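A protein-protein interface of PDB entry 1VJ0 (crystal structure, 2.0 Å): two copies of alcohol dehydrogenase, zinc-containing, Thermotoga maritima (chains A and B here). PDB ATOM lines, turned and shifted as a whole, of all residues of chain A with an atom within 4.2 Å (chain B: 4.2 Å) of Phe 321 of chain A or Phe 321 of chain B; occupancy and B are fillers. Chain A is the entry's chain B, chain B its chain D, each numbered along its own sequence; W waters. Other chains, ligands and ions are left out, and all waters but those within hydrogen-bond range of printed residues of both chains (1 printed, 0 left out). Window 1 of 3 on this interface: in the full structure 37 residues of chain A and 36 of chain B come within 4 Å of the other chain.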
ATOM      1  N   SER A 285     -31.847 -22.138 -12.858  1.00  0.00           N
ATOM      2  CA  SER A 285     -30.539 -22.217 -12.183  1.00  0.00           C
ATOM      3  C   SER A 285     -30.599 -21.820 -10.710  1.00  0.00           C
ATOM      4  O   SER A 285     -29.868 -22.376  -9.880  1.00  0.00           O
ATOM      5  CB  SER A 285     -29.472 -21.440 -12.935  1.00  0.00           C
ATOM      6  OG  SER A 285     -29.315 -21.921 -14.247  1.00  0.00           O
ATOM      7  N   TYR A 294     -29.466 -30.499 -14.038  1.00  0.00           N
ATOM      8  CA  TYR A 294     -30.424 -29.797 -14.907  1.00  0.00           C
ATOM      9  C   TYR A 294     -30.353 -30.381 -16.329  1.00  0.00           C
ATOM     10  O   TYR A 294     -29.352 -30.197 -17.009  1.00  0.00           O
ATOM     11  CB  TYR A 294     -29.995 -28.343 -14.912  1.00  0.00           C
ATOM     12  CG  TYR A 294     -30.993 -27.311 -15.261  1.00  0.00           C
ATOM     13  CD1 TYR A 294     -32.132 -27.581 -16.014  1.00  0.00           C
ATOM     14  CD2 TYR A 294     -30.787 -26.014 -14.866  1.00  0.00           C
ATOM     15  CE1 TYR A 294     -33.041 -26.574 -16.308  1.00  0.00           C
ATOM     16  CE2 TYR A 294     -31.638 -25.017 -15.222  1.00  0.00           C
ATOM     17  CZ  TYR A 294     -32.776 -25.300 -15.936  1.00  0.00           C
ATOM     18  OH  TYR A 294     -33.630 -24.264 -16.243  1.00  0.00           O
ATOM     19  N   PHE A 308     -25.205 -16.050 -18.505  1.00  0.00           N
ATOM     20  CA  PHE A 308     -24.989 -17.198 -17.670  1.00  0.00           C
ATOM     21  C   PHE A 308     -23.959 -16.887 -16.594  1.00  0.00           C
ATOM     22  O   PHE A 308     -22.862 -16.448 -16.885  1.00  0.00           O
ATOM     23  CB  PHE A 308     -24.553 -18.372 -18.537  1.00  0.00           C
ATOM     24  CG  PHE A 308     -24.562 -19.666 -17.798  1.00  0.00           C
ATOM     25  CD1 PHE A 308     -23.468 -20.034 -17.005  1.00  0.00           C
ATOM     26  CD2 PHE A 308     -25.649 -20.495 -17.841  1.00  0.00           C
ATOM     27  CE1 PHE A 308     -23.498 -21.195 -16.247  1.00  0.00           C
ATOM     28  CE2 PHE A 308     -25.658 -21.694 -17.108  1.00  0.00           C
ATOM     29  CZ  PHE A 308     -24.596 -22.030 -16.322  1.00  0.00           C
ATOM     30  N   TRP A 313     -23.790 -20.344 -10.771  1.00  0.00           N
ATOM     31  CA  TRP A 313     -24.697 -21.399 -11.247  1.00  0.00           C
ATOM     32  C   TRP A 313     -24.041 -22.729 -11.576  1.00  0.00           C
ATOM     33  O   TRP A 313     -24.734 -23.766 -11.532  1.00  0.00           O
ATOM     34  CB  TRP A 313     -25.501 -20.914 -12.462  1.00  0.00           C
ATOM     35  CG  TRP A 313     -26.374 -19.812 -12.131  1.00  0.00           C
ATOM     36  CD1 TRP A 313     -26.712 -19.360 -10.890  1.00  0.00           C
ATOM     37  CD2 TRP A 313     -27.062 -18.985 -13.060  1.00  0.00           C
ATOM     38  NE1 TRP A 313     -27.554 -18.277 -11.001  1.00  0.00           N
ATOM     39  CE2 TRP A 313     -27.801 -18.049 -12.327  1.00  0.00           C
ATOM     40  CE3 TRP A 313     -27.158 -18.969 -14.448  1.00  0.00           C
ATOM     41  CZ2 TRP A 313     -28.638 -17.112 -12.937  1.00  0.00           C
ATOM     42  CZ3 TRP A 313     -27.986 -18.022 -15.058  1.00  0.00           C
ATOM     43  CH2 TRP A 313     -28.690 -17.102 -14.306  1.00  0.00           C
ATOM     44  N   LEU A 314     -22.733 -22.720 -11.851  1.00  0.00           N
ATOM     45  CA  LEU A 314     -22.029 -23.975 -12.175  1.00  0.00           C
ATOM     46  C   LEU A 314     -21.030 -24.360 -11.101  1.00  0.00           C
ATOM     47  O   LEU A 314     -21.169 -25.390 -10.471  1.00  0.00           O
ATOM     48  CB  LEU A 314     -21.267 -23.880 -13.526  1.00  0.00           C
ATOM     49  CG  LEU A 314     -21.840 -24.512 -14.786  1.00  0.00           C
ATOM     50  CD1 LEU A 314     -20.853 -24.171 -15.946  1.00  0.00           C
ATOM     51  CD2 LEU A 314     -22.116 -25.993 -14.674  1.00  0.00           C
ATOM     52  N   ALA A 319     -22.898 -27.923 -10.059  1.00  0.00           N
ATOM     53  CA  ALA A 319     -24.079 -28.412 -10.743  1.00  0.00           C
ATOM     54  C   ALA A 319     -23.723 -29.133 -12.059  1.00  0.00           C
ATOM     55  O   ALA A 319     -22.660 -28.863 -12.632  1.00  0.00           O
ATOM     56  CB  ALA A 319     -24.981 -27.240 -11.021  1.00  0.00           C
ATOM     57  N   THR A 320     -24.603 -30.040 -12.508  1.00  0.00           N
ATOM     58  CA  THR A 320     -24.543 -30.612 -13.854  1.00  0.00           C
ATOM     59  C   THR A 320     -25.596 -30.000 -14.736  1.00  0.00           C
ATOM     60  O   THR A 320     -26.769 -30.009 -14.378  1.00  0.00           O
ATOM     61  CB  THR A 320     -24.732 -32.108 -13.819  1.00  0.00           C
ATOM     62  OG1 THR A 320     -23.765 -32.676 -12.938  1.00  0.00           O
ATOM     63  CG2 THR A 320     -24.420 -32.744 -15.191  1.00  0.00           C
ATOM     64  N   PHE A 321     -25.182 -29.416 -15.852  1.00  0.00           N
ATOM     65  CA  PHE A 321     -26.095 -29.028 -16.891  1.00  0.00           C
ATOM     66  C   PHE A 321     -25.897 -30.017 -18.029  1.00  0.00           C
ATOM     67  O   PHE A 321     -24.760 -30.156 -18.535  1.00  0.00           O
ATOM     68  CB  PHE A 321     -25.853 -27.604 -17.367  1.00  0.00           C
ATOM     69  CG  PHE A 321     -26.357 -26.557 -16.425  1.00  0.00           C
ATOM     70  CD1 PHE A 321     -25.779 -26.379 -15.172  1.00  0.00           C
ATOM     71  CD2 PHE A 321     -27.391 -25.687 -16.813  1.00  0.00           C
ATOM     72  CE1 PHE A 321     -26.210 -25.335 -14.316  1.00  0.00           C
ATOM     73  CE2 PHE A 321     -27.841 -24.686 -15.956  1.00  0.00           C
ATOM     74  CZ  PHE A 321     -27.249 -24.515 -14.700  1.00  0.00           C
ATOM     75  N   LYS A 322     -26.987 -30.707 -18.423  1.00  0.00           N
ATOM     76  CA  LYS A 322     -26.924 -31.713 -19.445  1.00  0.00           C
ATOM     77  C   LYS A 322     -27.883 -31.431 -20.550  1.00  0.00           C
ATOM     78  O   LYS A 322     -29.084 -31.492 -20.340  1.00  0.00           O
ATOM     79  CB  LYS A 322     -27.267 -33.082 -18.849  1.00  0.00           C
ATOM     80  CG  LYS A 322     -27.268 -34.219 -19.780  1.00  0.00           C
ATOM     81  CD  LYS A 322     -25.947 -34.717 -20.114  1.00  0.00           C
ATOM     82  CE  LYS A 322     -25.964 -35.395 -21.429  1.00  0.00           C
ATOM     83  NZ  LYS A 322     -24.604 -35.691 -21.867  1.00  0.00           N
ATOM     84  N   GLY A 323     -27.350 -31.152 -21.741  1.00  0.00           N
ATOM     85  CA  GLY A 323     -28.152 -30.970 -22.923  1.00  0.00           C
ATOM     86  C   GLY A 323     -28.626 -32.366 -23.440  1.00  0.00           C
ATOM     87  O   GLY A 323     -27.863 -33.356 -23.427  1.00  0.00           O
ATOM     88  N   SER B 285     -16.461 -24.179 -25.400  1.00  0.00           N
ATOM     89  CA  SER B 285     -17.687 -24.773 -25.964  1.00  0.00           C
ATOM     90  C   SER B 285     -17.563 -25.134 -27.439  1.00  0.00           C
ATOM     91  O   SER B 285     -18.118 -26.144 -27.849  1.00  0.00           O
ATOM     92  CB  SER B 285     -18.897 -23.871 -25.759  1.00  0.00           C
ATOM     93  OG  SER B 285     -19.189 -23.799 -24.379  1.00  0.00           O
ATOM     94  N   TYR B 294     -17.474 -31.093 -20.124  1.00  0.00           N
ATOM     95  CA  TYR B 294     -16.721 -29.908 -19.815  1.00  0.00           C
ATOM     96  C   TYR B 294     -16.746 -29.741 -18.295  1.00  0.00           C
ATOM     97  O   TYR B 294     -17.806 -29.461 -17.761  1.00  0.00           O
ATOM     98  CB  TYR B 294     -17.403 -28.747 -20.524  1.00  0.00           C
ATOM     99  CG  TYR B 294     -16.616 -27.516 -20.781  1.00  0.00           C
ATOM    100  CD1 TYR B 294     -15.431 -27.225 -20.107  1.00  0.00           C
ATOM    101  CD2 TYR B 294     -17.057 -26.589 -21.706  1.00  0.00           C
ATOM    102  CE1 TYR B 294     -14.719 -26.061 -20.356  1.00  0.00           C
ATOM    103  CE2 TYR B 294     -16.341 -25.413 -21.944  1.00  0.00           C
ATOM    104  CZ  TYR B 294     -15.175 -25.170 -21.276  1.00  0.00           C
ATOM    105  OH  TYR B 294     -14.486 -24.011 -21.512  1.00  0.00           O
ATOM    106  N   PHE B 308     -24.325 -17.219 -23.118  1.00  0.00           N
ATOM    107  CA  PHE B 308     -24.311 -18.696 -23.268  1.00  0.00           C
ATOM    108  C   PHE B 308     -25.365 -19.109 -24.290  1.00  0.00           C
ATOM    109  O   PHE B 308     -26.511 -18.797 -24.138  1.00  0.00           O
ATOM    110  CB  PHE B 308     -24.559 -19.365 -21.910  1.00  0.00           C
ATOM    111  CG  PHE B 308     -24.340 -20.868 -21.916  1.00  0.00           C
ATOM    112  CD1 PHE B 308     -25.278 -21.714 -22.436  1.00  0.00           C
ATOM    113  CD2 PHE B 308     -23.179 -21.416 -21.415  1.00  0.00           C
ATOM    114  CE1 PHE B 308     -25.056 -23.103 -22.448  1.00  0.00           C
ATOM    115  CE2 PHE B 308     -22.965 -22.797 -21.435  1.00  0.00           C
ATOM    116  CZ  PHE B 308     -23.881 -23.619 -21.956  1.00  0.00           C
ATOM    117  N   TRP B 313     -24.488 -24.976 -27.603  1.00  0.00           N
ATOM    118  CA  TRP B 313     -23.482 -25.537 -26.724  1.00  0.00           C
ATOM    119  C   TRP B 313     -23.963 -26.631 -25.821  1.00  0.00           C
ATOM    120  O   TRP B 313     -23.138 -27.420 -25.369  1.00  0.00           O
ATOM    121  CB  TRP B 313     -22.914 -24.449 -25.848  1.00  0.00           C
ATOM    122  CG  TRP B 313     -22.249 -23.439 -26.675  1.00  0.00           C
ATOM    123  CD1 TRP B 313     -21.864 -23.562 -27.995  1.00  0.00           C
ATOM    124  CD2 TRP B 313     -21.794 -22.184 -26.244  1.00  0.00           C
ATOM    125  NE1 TRP B 313     -21.214 -22.422 -28.384  1.00  0.00           N
ATOM    126  CE2 TRP B 313     -21.128 -21.584 -27.314  1.00  0.00           C
ATOM    127  CE3 TRP B 313     -21.812 -21.529 -25.027  1.00  0.00           C
ATOM    128  CZ2 TRP B 313     -20.614 -20.317 -27.240  1.00  0.00           C
ATOM    129  CZ3 TRP B 313     -21.272 -20.276 -24.955  1.00  0.00           C
ATOM    130  CH2 TRP B 313     -20.681 -19.696 -26.035  1.00  0.00           C
ATOM    131  N   LEU B 314     -25.269 -26.670 -25.541  1.00  0.00           N
ATOM    132  CA  LEU B 314     -25.813 -27.670 -24.646  1.00  0.00           C
ATOM    133  C   LEU B 314     -26.704 -28.674 -25.359  1.00  0.00           C
ATOM    134  O   LEU B 314     -26.371 -29.845 -25.394  1.00  0.00           O
ATOM    135  CB  LEU B 314     -26.601 -27.017 -23.517  1.00  0.00           C
ATOM    136  CG  LEU B 314     -26.066 -26.863 -22.128  1.00  0.00           C
ATOM    137  CD1 LEU B 314     -27.226 -26.289 -21.295  1.00  0.00           C
ATOM    138  CD2 LEU B 314     -25.492 -28.158 -21.509  1.00  0.00           C
ATOM    139  N   ALA B 319     -24.155 -31.995 -24.595  1.00  0.00           N
ATOM    140  CA  ALA B 319     -22.960 -31.795 -23.804  1.00  0.00           C
ATOM    141  C   ALA B 319     -23.275 -31.837 -22.289  1.00  0.00           C
ATOM    142  O   ALA B 319     -24.391 -31.554 -21.878  1.00  0.00           O
ATOM    143  CB  ALA B 319     -22.330 -30.453 -24.178  1.00  0.00           C
ATOM    144  N   THR B 320     -22.293 -32.233 -21.486  1.00  0.00           N
ATOM    145  CA  THR B 320     -22.318 -32.049 -20.021  1.00  0.00           C
ATOM    146  C   THR B 320     -21.393 -30.946 -19.609  1.00  0.00           C
ATOM    147  O   THR B 320     -20.214 -31.007 -19.932  1.00  0.00           O
ATOM    148  CB  THR B 320     -21.845 -33.335 -19.329  1.00  0.00           C
ATOM    149  OG1 THR B 320     -22.665 -34.428 -19.762  1.00  0.00           O
ATOM    150  CG2 THR B 320     -22.005 -33.259 -17.778  1.00  0.00           C
ATOM    151  N   PHE B 321     -21.926 -29.938 -18.906  1.00  0.00           N
ATOM    152  CA  PHE B 321     -21.153 -28.903 -18.267  1.00  0.00           C
ATOM    153  C   PHE B 321     -21.287 -29.213 -16.793  1.00  0.00           C
ATOM    154  O   PHE B 321     -22.413 -29.317 -16.277  1.00  0.00           O
ATOM    155  CB  PHE B 321     -21.658 -27.497 -18.558  1.00  0.00           C
ATOM    156  CG  PHE B 321     -21.340 -26.993 -19.949  1.00  0.00           C
ATOM    157  CD1 PHE B 321     -21.872 -27.611 -21.067  1.00  0.00           C
ATOM    158  CD2 PHE B 321     -20.532 -25.871 -20.123  1.00  0.00           C
ATOM    159  CE1 PHE B 321     -21.596 -27.101 -22.349  1.00  0.00           C
ATOM    160  CE2 PHE B 321     -20.245 -25.367 -21.355  1.00  0.00           C
ATOM    161  CZ  PHE B 321     -20.781 -25.984 -22.496  1.00  0.00           C
ATOM    162  N   LYS B 322     -20.151 -29.456 -16.149  1.00  0.00           N
ATOM    163  CA  LYS B 322     -20.112 -29.817 -14.743  1.00  0.00           C
ATOM    164  C   LYS B 322     -19.260 -28.854 -13.968  1.00  0.00           C
ATOM    165  O   LYS B 322     -18.028 -28.816 -14.156  1.00  0.00           O
ATOM    166  CB  LYS B 322     -19.502 -31.207 -14.632  1.00  0.00           C
ATOM    167  CG  LYS B 322     -19.351 -31.803 -13.261  1.00  0.00           C
ATOM    168  CD  LYS B 322     -20.662 -32.056 -12.640  1.00  0.00           C
ATOM    169  CE  LYS B 322     -20.528 -32.335 -11.183  1.00  0.00           C
ATOM    170  NZ  LYS B 322     -21.846 -32.493 -10.577  1.00  0.00           N
ATOM    171  N   GLY B 323     -19.886 -28.109 -13.059  1.00  0.00           N
ATOM    172  CA  GLY B 323     -19.121 -27.284 -12.166  1.00  0.00           C
ATOM    173  C   GLY B 323     -18.436 -28.136 -11.123  1.00  0.00           C
ATOM    174  O   GLY B 323     -18.991 -29.123 -10.642  1.00  0.00           O
HETATM  175  O   HOH W   1     -21.158 -35.759 -21.754  1.00  0.00           O
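OG1 of Thr 320 of chain A sits at hydrogen-bond distance from NZ of Lys 322 of chain B (3.0 Å).
The backbone carbonyl oxygen of Ala 319 of chain A is in hydrogen-bond range of the backbone NH of Gly 323 of chain B, at 2.9 Å.
The backbone NH (N) of Gly 323 of chain A is in hydrogen-bond range of the backbone carbonyl oxygen (O) of Ala 319 of chain B, at 3.0 Å.
The side-chain amino group (NZ) of Lys 322 of chain A is in hydrogen-bond range of the side-chain hydroxyl (OG1) of Thr 320 of chain B.
N of Phe 321 of chain A lies within hydrogen-bond range of O of Phe 321 of chain B (2.8 Å).
The backbone carbonyl oxygen (O) of Tyr 294 of chain A lies within hydrogen-bond range of the backbone NH (N) of Lys 322 of chain A.
N of Tyr 294 of chain A is in hydrogen-bond range of O of Thr 320 of chain A.
The backbone carbonyl oxygen of Tyr 294 of chain B lies within hydrogen-bond range of the backbone NH of Lys 322 of chain B (2.8 Å).
O of Thr 320 of chain B is in hydrogen-bond range of N of Tyr 294 of chain B, at 2.7 Å.
O of Leu 314 of chain B is in hydrogen-bond range of N of Ala 319 of chain B, 3.2 Å away.
The backbone NH of Ala 319 of chain A is in hydrogen-bond range of the backbone carbonyl oxygen of Leu 314 of chain A, at 3.1 Å.
Among the printed residues, merely in contact across the chains: Gly 323 of chain A with Leu 314 of chain B, Leu 314 of chain A with Gly 323 of chain B, Phe 321 of chain A with Thr 320 of chain B, Ala 319 of chain A with Lys 322 of chain B, Thr 320 of chain A with Phe 321 of chain B, Lys 322 of chain A with Ala 319 of chain B, Phe 308 of chain A with Phe 308 of chain B, Thr 320 of chain A with Thr 320 of chain B, Phe 321 of chain A with Ala 319 of chain B, Phe 321 of chain A with Leu 314 of chain B, Ala 319 of chain A with Phe 321 of chain B and Leu 314 of chain A with Phe 321 of chain B.
Of the printed residues of chain B, Phe 321 of chain A touches Leu 314 (3.7 Å), Ala 319 (3.6 Å), Thr 320 (3.4 Å) and Phe 321 (2.8 Å).
Phe 321 of chain B touches four residues of chain A.
Of the printed residues of chain A, Thr 320 of chain B touches Thr 320, Phe 321 and Lys 322.
Printed residues of chain B within 4 Å of Thr 320 of chain A: Thr 320, Phe 321 and Lys 322.
Printed residues of chain B within 4 Å of Ala 319 of chain A: Phe 321, Lys 322 and Gly 323.
Trp 313 of chain B touches none of the printed residues of chain A.
The nearest printed residue of chain B that does not touch Phe 321 of chain A is Lys 322 of chain B (5.0 Å).
The nearest printed residue of chain A that does not touch Phe 308 of chain B is Leu 314 of chain A (6.0 Å).
Hydrophobic or aromatic side chains of chain B that line the printed part of chain A: Phe 308 and Leu 314.
Hydrophobic or aromatic side chains of chain A within 4 Å of the printed part of chain B: Phe 308, Leu 314 and Phe 321.
Along chain A the printed residues that touch a printed residue of chain B span positions 308 to 323.
Among the printed residues, no Asp or Glu carboxylate lies within 4 Å of a Lys or Arg side-chain nitrogen of the other chain.
Leu 314 of chain A touches Phe 321 of chain B, and with the chains exchanged Phe 321 of chain A touches Leu 314 of chain B.
Ala 319 of chain A touches Gly 323 of chain B, and with the chains exchanged Gly 323 of chain A touches Ala 319 of chain B.
Thr 320 of chain A touches Lys 322 of chain B, and with the chains exchanged Lys 322 of chain A touches Thr 320 of chain B.
Phe 321 of chain B touches its own counterpart, Phe 321 of chain A.
Positions printed for both chains: 285, 294, 308, 313, 314, 319, 320, 321, 322 and 323.
Of the 17 pairs that touch across the chains among the printed residues, 17 have their exchanged pair printed and touching as well.
Water W1 bridges OG1 of Thr 320 of chain B and NZ of Lys 322 of chain A.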
